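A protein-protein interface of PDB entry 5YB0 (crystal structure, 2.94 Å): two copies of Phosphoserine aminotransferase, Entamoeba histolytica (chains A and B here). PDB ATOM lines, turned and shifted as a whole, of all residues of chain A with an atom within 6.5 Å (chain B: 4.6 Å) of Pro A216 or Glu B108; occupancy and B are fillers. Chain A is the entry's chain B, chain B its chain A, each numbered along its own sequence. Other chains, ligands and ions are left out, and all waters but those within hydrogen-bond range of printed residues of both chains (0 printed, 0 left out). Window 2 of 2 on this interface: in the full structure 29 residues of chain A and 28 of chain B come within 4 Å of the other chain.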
ATOM      1  N   MET A  86      -5.040  -6.994 -27.713  1.00  0.00           N
ATOM      2  CA  MET A  86      -4.471  -5.856 -27.022  1.00  0.00           C
ATOM      3  C   MET A  86      -3.142  -5.471 -27.652  1.00  0.00           C
ATOM      4  O   MET A  86      -2.845  -4.297 -27.768  1.00  0.00           O
ATOM      5  CB  MET A  86      -4.296  -6.160 -25.537  1.00  0.00           C
ATOM      6  CG  MET A  86      -5.611  -6.415 -24.803  1.00  0.00           C
ATOM      7  SD  MET A  86      -5.679  -5.590 -23.200  1.00  0.00           S
ATOM      8  CE  MET A  86      -5.806  -3.902 -23.802  1.00  0.00           C
ATOM      9  N   LYS A 214      -2.079   1.495 -25.360  1.00  0.00           N
ATOM     10  CA  LYS A 214      -2.722   1.087 -24.103  1.00  0.00           C
ATOM     11  C   LYS A 214      -2.603  -0.378 -23.579  1.00  0.00           C
ATOM     12  O   LYS A 214      -3.582  -1.122 -23.665  1.00  0.00           O
ATOM     13  CB  LYS A 214      -4.209   1.441 -24.373  1.00  0.00           C
ATOM     14  CG  LYS A 214      -4.685   0.914 -25.764  1.00  0.00           C
ATOM     15  CD  LYS A 214      -5.934   0.035 -25.834  1.00  0.00           C
ATOM     16  CE  LYS A 214      -5.759  -1.086 -26.873  1.00  0.00           C
ATOM     17  NZ  LYS A 214      -6.811  -1.086 -27.926  1.00  0.00           N
ATOM     18  N   ILE A 215      -1.472  -0.789 -22.984  1.00  0.00           N
ATOM     19  CA  ILE A 215      -1.271  -2.231 -22.622  1.00  0.00           C
ATOM     20  C   ILE A 215      -0.730  -2.532 -21.218  1.00  0.00           C
ATOM     21  O   ILE A 215       0.374  -2.104 -20.886  1.00  0.00           O
ATOM     22  CB  ILE A 215      -0.291  -2.942 -23.586  1.00  0.00           C
ATOM     23  CG1 ILE A 215      -0.737  -2.772 -25.019  1.00  0.00           C
ATOM     24  CG2 ILE A 215      -0.215  -4.437 -23.268  1.00  0.00           C
ATOM     25  CD1 ILE A 215       0.150  -3.477 -25.998  1.00  0.00           C
ATOM     26  N   PRO A 216      -1.450  -3.347 -20.425  1.00  0.00           N
ATOM     27  CA  PRO A 216      -0.943  -3.630 -19.096  1.00  0.00           C
ATOM     28  C   PRO A 216       0.280  -4.470 -19.154  1.00  0.00           C
ATOM     29  O   PRO A 216       0.399  -5.324 -20.033  1.00  0.00           O
ATOM     30  CB  PRO A 216      -2.048  -4.436 -18.434  1.00  0.00           C
ATOM     31  CG  PRO A 216      -3.203  -4.380 -19.322  1.00  0.00           C
ATOM     32  CD  PRO A 216      -2.717  -4.029 -20.684  1.00  0.00           C
ATOM     33  N   ILE A 217       1.171  -4.271 -18.200  1.00  0.00           N
ATOM     34  CA  ILE A 217       2.488  -4.903 -18.264  1.00  0.00           C
ATOM     35  C   ILE A 217       2.338  -6.382 -18.484  1.00  0.00           C
ATOM     36  O   ILE A 217       3.009  -6.938 -19.313  1.00  0.00           O
ATOM     37  CB  ILE A 217       3.314  -4.639 -16.997  1.00  0.00           C
ATOM     38  CG1 ILE A 217       3.729  -3.164 -16.936  1.00  0.00           C
ATOM     39  CG2 ILE A 217       4.544  -5.504 -16.965  1.00  0.00           C
ATOM     40  CD1 ILE A 217       4.069  -2.704 -15.537  1.00  0.00           C
ATOM     41  N   ILE A 218       1.435  -7.017 -17.760  1.00  0.00           N
ATOM     42  CA  ILE A 218       1.365  -8.474 -17.742  1.00  0.00           C
ATOM     43  C   ILE A 218       0.828  -9.020 -19.058  1.00  0.00           C
ATOM     44  O   ILE A 218       0.956 -10.206 -19.315  1.00  0.00           O
ATOM     45  CB  ILE A 218       0.500  -8.945 -16.534  1.00  0.00           C
ATOM     46  CG1 ILE A 218       0.933 -10.312 -15.933  1.00  0.00           C
ATOM     47  CG2 ILE A 218      -0.997  -8.880 -16.848  1.00  0.00           C
ATOM     48  CD1 ILE A 218       2.035 -11.078 -16.621  1.00  0.00           C
ATOM     49  N   LEU A 219       0.216  -8.168 -19.878  1.00  0.00           N
ATOM     50  CA  LEU A 219      -0.376  -8.601 -21.140  1.00  0.00           C
ATOM     51  C   LEU A 219       0.472  -8.242 -22.357  1.00  0.00           C
ATOM     52  O   LEU A 219       0.036  -8.354 -23.511  1.00  0.00           O
ATOM     53  CB  LEU A 219      -1.790  -8.000 -21.288  1.00  0.00           C
ATOM     54  CG  LEU A 219      -2.871  -8.394 -20.283  1.00  0.00           C
ATOM     55  CD1 LEU A 219      -4.232  -7.960 -20.778  1.00  0.00           C
ATOM     56  CD2 LEU A 219      -2.882  -9.882 -19.981  1.00  0.00           C
ATOM     57  N   ASP A 220       1.700  -7.821 -22.107  1.00  0.00           N
ATOM     58  CA  ASP A 220       2.523  -7.197 -23.147  1.00  0.00           C
ATOM     59  C   ASP A 220       3.513  -8.208 -23.692  1.00  0.00           C
ATOM     60  O   ASP A 220       4.506  -8.471 -23.043  1.00  0.00           O
ATOM     61  CB  ASP A 220       3.256  -5.996 -22.539  1.00  0.00           C
ATOM     62  CG  ASP A 220       4.080  -5.242 -23.549  1.00  0.00           C
ATOM     63  OD1 ASP A 220       4.570  -5.900 -24.472  1.00  0.00           O
ATOM     64  OD2 ASP A 220       4.269  -4.000 -23.425  1.00  0.00           O
ATOM     65  N   VAL A 223       7.117  -7.259 -23.246  1.00  0.00           N
ATOM     66  CA  VAL A 223       7.686  -7.443 -21.911  1.00  0.00           C
ATOM     67  C   VAL A 223       8.140  -8.885 -21.688  1.00  0.00           C
ATOM     68  O   VAL A 223       9.194  -9.133 -21.118  1.00  0.00           O
ATOM     69  CB  VAL A 223       6.660  -7.084 -20.799  1.00  0.00           C
ATOM     70  CG1 VAL A 223       7.172  -7.531 -19.436  1.00  0.00           C
ATOM     71  CG2 VAL A 223       6.383  -5.586 -20.773  1.00  0.00           C
ATOM     72  N   TYR A 231       9.107 -13.166 -17.152  1.00  0.00           N
ATOM     73  CA  TYR A 231       8.900 -11.839 -16.564  1.00  0.00           C
ATOM     74  C   TYR A 231       8.401 -12.115 -15.182  1.00  0.00           C
ATOM     75  O   TYR A 231       8.949 -11.589 -14.232  1.00  0.00           O
ATOM     76  CB  TYR A 231       7.883 -10.994 -17.360  1.00  0.00           C
ATOM     77  CG  TYR A 231       7.302  -9.880 -16.542  1.00  0.00           C
ATOM     78  CD1 TYR A 231       8.031  -8.743 -16.280  1.00  0.00           C
ATOM     79  CD2 TYR A 231       6.020  -9.982 -16.009  1.00  0.00           C
ATOM     80  CE1 TYR A 231       7.509  -7.715 -15.508  1.00  0.00           C
ATOM     81  CE2 TYR A 231       5.483  -8.971 -15.238  1.00  0.00           C
ATOM     82  CZ  TYR A 231       6.248  -7.843 -14.972  1.00  0.00           C
ATOM     83  OH  TYR A 231       5.746  -6.833 -14.185  1.00  0.00           O
ATOM     84  N   PHE B  81      -2.351  -8.715 -10.427  1.00  0.00           N
ATOM     85  CA  PHE B  81      -2.128  -7.279 -10.235  1.00  0.00           C
ATOM     86  C   PHE B  81      -3.034  -6.505 -11.142  1.00  0.00           C
ATOM     87  O   PHE B  81      -3.608  -5.539 -10.743  1.00  0.00           O
ATOM     88  CB  PHE B  81      -0.696  -6.860 -10.499  1.00  0.00           C
ATOM     89  CG  PHE B  81       0.305  -7.382  -9.489  1.00  0.00           C
ATOM     90  CD1 PHE B  81      -0.075  -7.769  -8.237  1.00  0.00           C
ATOM     91  CD2 PHE B  81       1.655  -7.450  -9.832  1.00  0.00           C
ATOM     92  CE1 PHE B  81       0.855  -8.225  -7.364  1.00  0.00           C
ATOM     93  CE2 PHE B  81       2.595  -7.880  -8.951  1.00  0.00           C
ATOM     94  CZ  PHE B  81       2.198  -8.274  -7.716  1.00  0.00           C
ATOM     95  N   LEU B  82      -3.168  -6.958 -12.368  1.00  0.00           N
ATOM     96  CA  LEU B  82      -4.098  -6.372 -13.318  1.00  0.00           C
ATOM     97  C   LEU B  82      -5.539  -6.712 -12.987  1.00  0.00           C
ATOM     98  O   LEU B  82      -6.369  -5.810 -12.893  1.00  0.00           O
ATOM     99  CB  LEU B  82      -3.782  -6.869 -14.735  1.00  0.00           C
ATOM    100  CG  LEU B  82      -4.736  -6.447 -15.835  1.00  0.00           C
ATOM    101  CD1 LEU B  82      -4.853  -4.937 -15.904  1.00  0.00           C
ATOM    102  CD2 LEU B  82      -4.238  -7.017 -17.165  1.00  0.00           C
ATOM    103  N   LYS B 104       5.175  -3.243  -7.891  1.00  0.00           N
ATOM    104  CA  LYS B 104       4.727  -3.852  -9.095  1.00  0.00           C
ATOM    105  C   LYS B 104       3.235  -3.775  -9.145  1.00  0.00           C
ATOM    106  O   LYS B 104       2.663  -3.438 -10.198  1.00  0.00           O
ATOM    107  CB  LYS B 104       5.233  -5.297  -9.204  1.00  0.00           C
ATOM    108  CG  LYS B 104       6.682  -5.333  -9.663  1.00  0.00           C
ATOM    109  CD  LYS B 104       7.228  -6.714  -9.891  1.00  0.00           C
ATOM    110  CE  LYS B 104       8.455  -6.604 -10.784  1.00  0.00           C
ATOM    111  NZ  LYS B 104       9.123  -7.932 -10.937  1.00  0.00           N
ATOM    112  N   ALA B 105       2.586  -4.065  -8.019  1.00  0.00           N
ATOM    113  CA  ALA B 105       1.119  -4.039  -7.994  1.00  0.00           C
ATOM    114  C   ALA B 105       0.597  -2.670  -8.364  1.00  0.00           C
ATOM    115  O   ALA B 105      -0.415  -2.552  -8.999  1.00  0.00           O
ATOM    116  CB  ALA B 105       0.589  -4.441  -6.623  1.00  0.00           C
ATOM    117  N   ILE B 106       1.281  -1.640  -7.903  1.00  0.00           N
ATOM    118  CA  ILE B 106       0.848  -0.268  -8.072  1.00  0.00           C
ATOM    119  C   ILE B 106       1.024   0.138  -9.512  1.00  0.00           C
ATOM    120  O   ILE B 106       0.141   0.733 -10.100  1.00  0.00           O
ATOM    121  CB  ILE B 106       1.670   0.685  -7.160  1.00  0.00           C
ATOM    122  CG1 ILE B 106       1.282   0.503  -5.697  1.00  0.00           C
ATOM    123  CG2 ILE B 106       1.456   2.143  -7.549  1.00  0.00           C
ATOM    124  CD1 ILE B 106       2.335   0.977  -4.721  1.00  0.00           C
ATOM    125  N   LYS B 107       2.191  -0.150 -10.069  1.00  0.00           N
ATOM    126  CA  LYS B 107       2.517   0.309 -11.411  1.00  0.00           C
ATOM    127  C   LYS B 107       1.468  -0.265 -12.375  1.00  0.00           C
ATOM    128  O   LYS B 107       1.041   0.420 -13.311  1.00  0.00           O
ATOM    129  CB  LYS B 107       3.972  -0.053 -11.770  1.00  0.00           C
ATOM    130  CG  LYS B 107       4.419   0.297 -13.194  1.00  0.00           C
ATOM    131  CD  LYS B 107       4.800   1.762 -13.385  1.00  0.00           C
ATOM    132  CE  LYS B 107       3.656   2.612 -13.943  1.00  0.00           C
ATOM    133  NZ  LYS B 107       3.767   4.074 -13.593  1.00  0.00           N
ATOM    134  N   GLU B 108       1.015  -1.496 -12.120  1.00  0.00           N
ATOM    135  CA  GLU B 108      -0.083  -2.074 -12.930  1.00  0.00           C
ATOM    136  C   GLU B 108      -1.377  -1.324 -12.755  1.00  0.00           C
ATOM    137  O   GLU B 108      -2.003  -0.905 -13.751  1.00  0.00           O
ATOM    138  CB  GLU B 108      -0.356  -3.548 -12.628  1.00  0.00           C
ATOM    139  CG  GLU B 108       0.519  -4.500 -13.423  1.00  0.00           C
ATOM    140  CD  GLU B 108       0.198  -4.572 -14.888  1.00  0.00           C
ATOM    141  OE1 GLU B 108       0.335  -5.696 -15.435  1.00  0.00           O
ATOM    142  OE2 GLU B 108      -0.161  -3.530 -15.479  1.00  0.00           O
ATOM    143  N   ALA B 109      -1.780  -1.176 -11.500  1.00  0.00           N
ATOM    144  CA  ALA B 109      -2.990  -0.438 -11.166  1.00  0.00           C
ATOM    145  C   ALA B 109      -2.996   0.960 -11.782  1.00  0.00           C
ATOM    146  O   ALA B 109      -4.004   1.397 -12.371  1.00  0.00           O
ATOM    147  CB  ALA B 109      -3.161  -0.346  -9.685  1.00  0.00           C
ATOM    148  N   GLU B 110      -1.859   1.644 -11.689  1.00  0.00           N
ATOM    149  CA  GLU B 110      -1.703   2.980 -12.279  1.00  0.00           C
ATOM    150  C   GLU B 110      -1.963   2.987 -13.780  1.00  0.00           C
ATOM    151  O   GLU B 110      -2.375   3.993 -14.327  1.00  0.00           O
ATOM    152  CB  GLU B 110      -0.292   3.505 -12.009  1.00  0.00           C
ATOM    153  CG  GLU B 110      -0.044   3.873 -10.556  1.00  0.00           C
ATOM    154  CD  GLU B 110       1.375   4.322 -10.317  1.00  0.00           C
ATOM    155  OE1 GLU B 110       2.220   4.007 -11.199  1.00  0.00           O
ATOM    156  OE2 GLU B 110       1.624   5.008  -9.284  1.00  0.00           O
ATOM    157  N   ASN B 111      -1.667   1.879 -14.450  1.00  0.00           N
ATOM    158  CA  ASN B 111      -1.887   1.764 -15.893  1.00  0.00           C
ATOM    159  C   ASN B 111      -3.358   1.641 -16.249  1.00  0.00           C
ATOM    160  O   ASN B 111      -3.699   1.908 -17.375  1.00  0.00           O
ATOM    161  CB  ASN B 111      -1.081   0.580 -16.488  1.00  0.00           C
ATOM    162  CG  ASN B 111       0.444   0.760 -16.343  1.00  0.00           C
ATOM    163  OD1 ASN B 111       0.959   1.837 -15.947  1.00  0.00           O
ATOM    164  ND2 ASN B 111       1.181  -0.297 -16.706  1.00  0.00           N
ATOM    165  N   ILE B 112      -4.220   1.244 -15.305  1.00  0.00           N
ATOM    166  CA  ILE B 112      -5.689   1.108 -15.560  1.00  0.00           C
ATOM    167  C   ILE B 112      -6.528   2.286 -14.991  1.00  0.00           C
ATOM    168  O   ILE B 112      -7.542   2.662 -15.586  1.00  0.00           O
ATOM    169  CB  ILE B 112      -6.262  -0.198 -14.993  1.00  0.00           C
ATOM    170  CG1 ILE B 112      -6.141  -1.326 -15.984  1.00  0.00           C
ATOM    171  CG2 ILE B 112      -7.728  -0.061 -14.602  1.00  0.00           C
ATOM    172  CD1 ILE B 112      -4.740  -1.516 -16.473  1.00  0.00           C
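No position is printed for both chains.
NZ of Lys B107 lies within salt-bridge range of OE1 of Glu B110 (2.9 Å). The backbone carbonyl oxygen (O) of Lys B107 lies close to the side-chain amide oxygen (OD1) of Asn B111 (3.0 Å).
The side-chain carboxylate (OE2) of Glu B108 is in hydrogen-bond range of the backbone NH (N) of Ile A217. OE1 of Glu B108 is in hydrogen-bond range of N of Ile A218 (2.9 Å).
Of the 11 printed residues of chain B, 4 touch a printed residue of chain A. Hydrophobic or aromatic side chains of chain B that line the printed part of chain A: Leu B82. Hydrophobic or aromatic side chains of chain A within 4 Å of the printed part of chain B: Pro A216, Ile A217, Ile A218 and Leu A219. Along chain A the printed residues that touch a printed residue of chain B span positions 216 to 219. Among the printed residues, 8 pairs touch across the chains.
Pro A216 touches two residues of chain B. Glu B108 touches just these residues of chain A: Pro A216, Ile A217 and Ile A218. Printed residues of chain B within 4 Å of Ile A218: Leu B82 and Glu B108. Printed residues of chain A within 4 Å of Lys B107: Ile A217. Printed residues of chain A within 4 Å of Asn B111: Ile A217 (3.8 Å). Ile B106 touches none of the printed residues of chain A. Ala B109 touches none of the printed residues of chain A. The nearest residue of chain A that does not touch Glu B108 is Leu A219 (5.1 Å). The nearest printed residue of chain A that does not touch Leu B82 is Ile A217 (6.2 Å).
CG of Pro A216 touches CD2 of Leu B82, 3.6 Å away. Glu B108 touches Pro A216 (OE2 to CB, 3.6 Å). Ile A217 touches Lys B107. Ile A217 touches Asn B111 (CG1 to ND2, 3.8 Å). CG2 of Ile A218 touches CD2 of Leu B82, 3.8 Å away. CD2 of Leu B82 touches CG of Leu A219 (3.7 Å).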
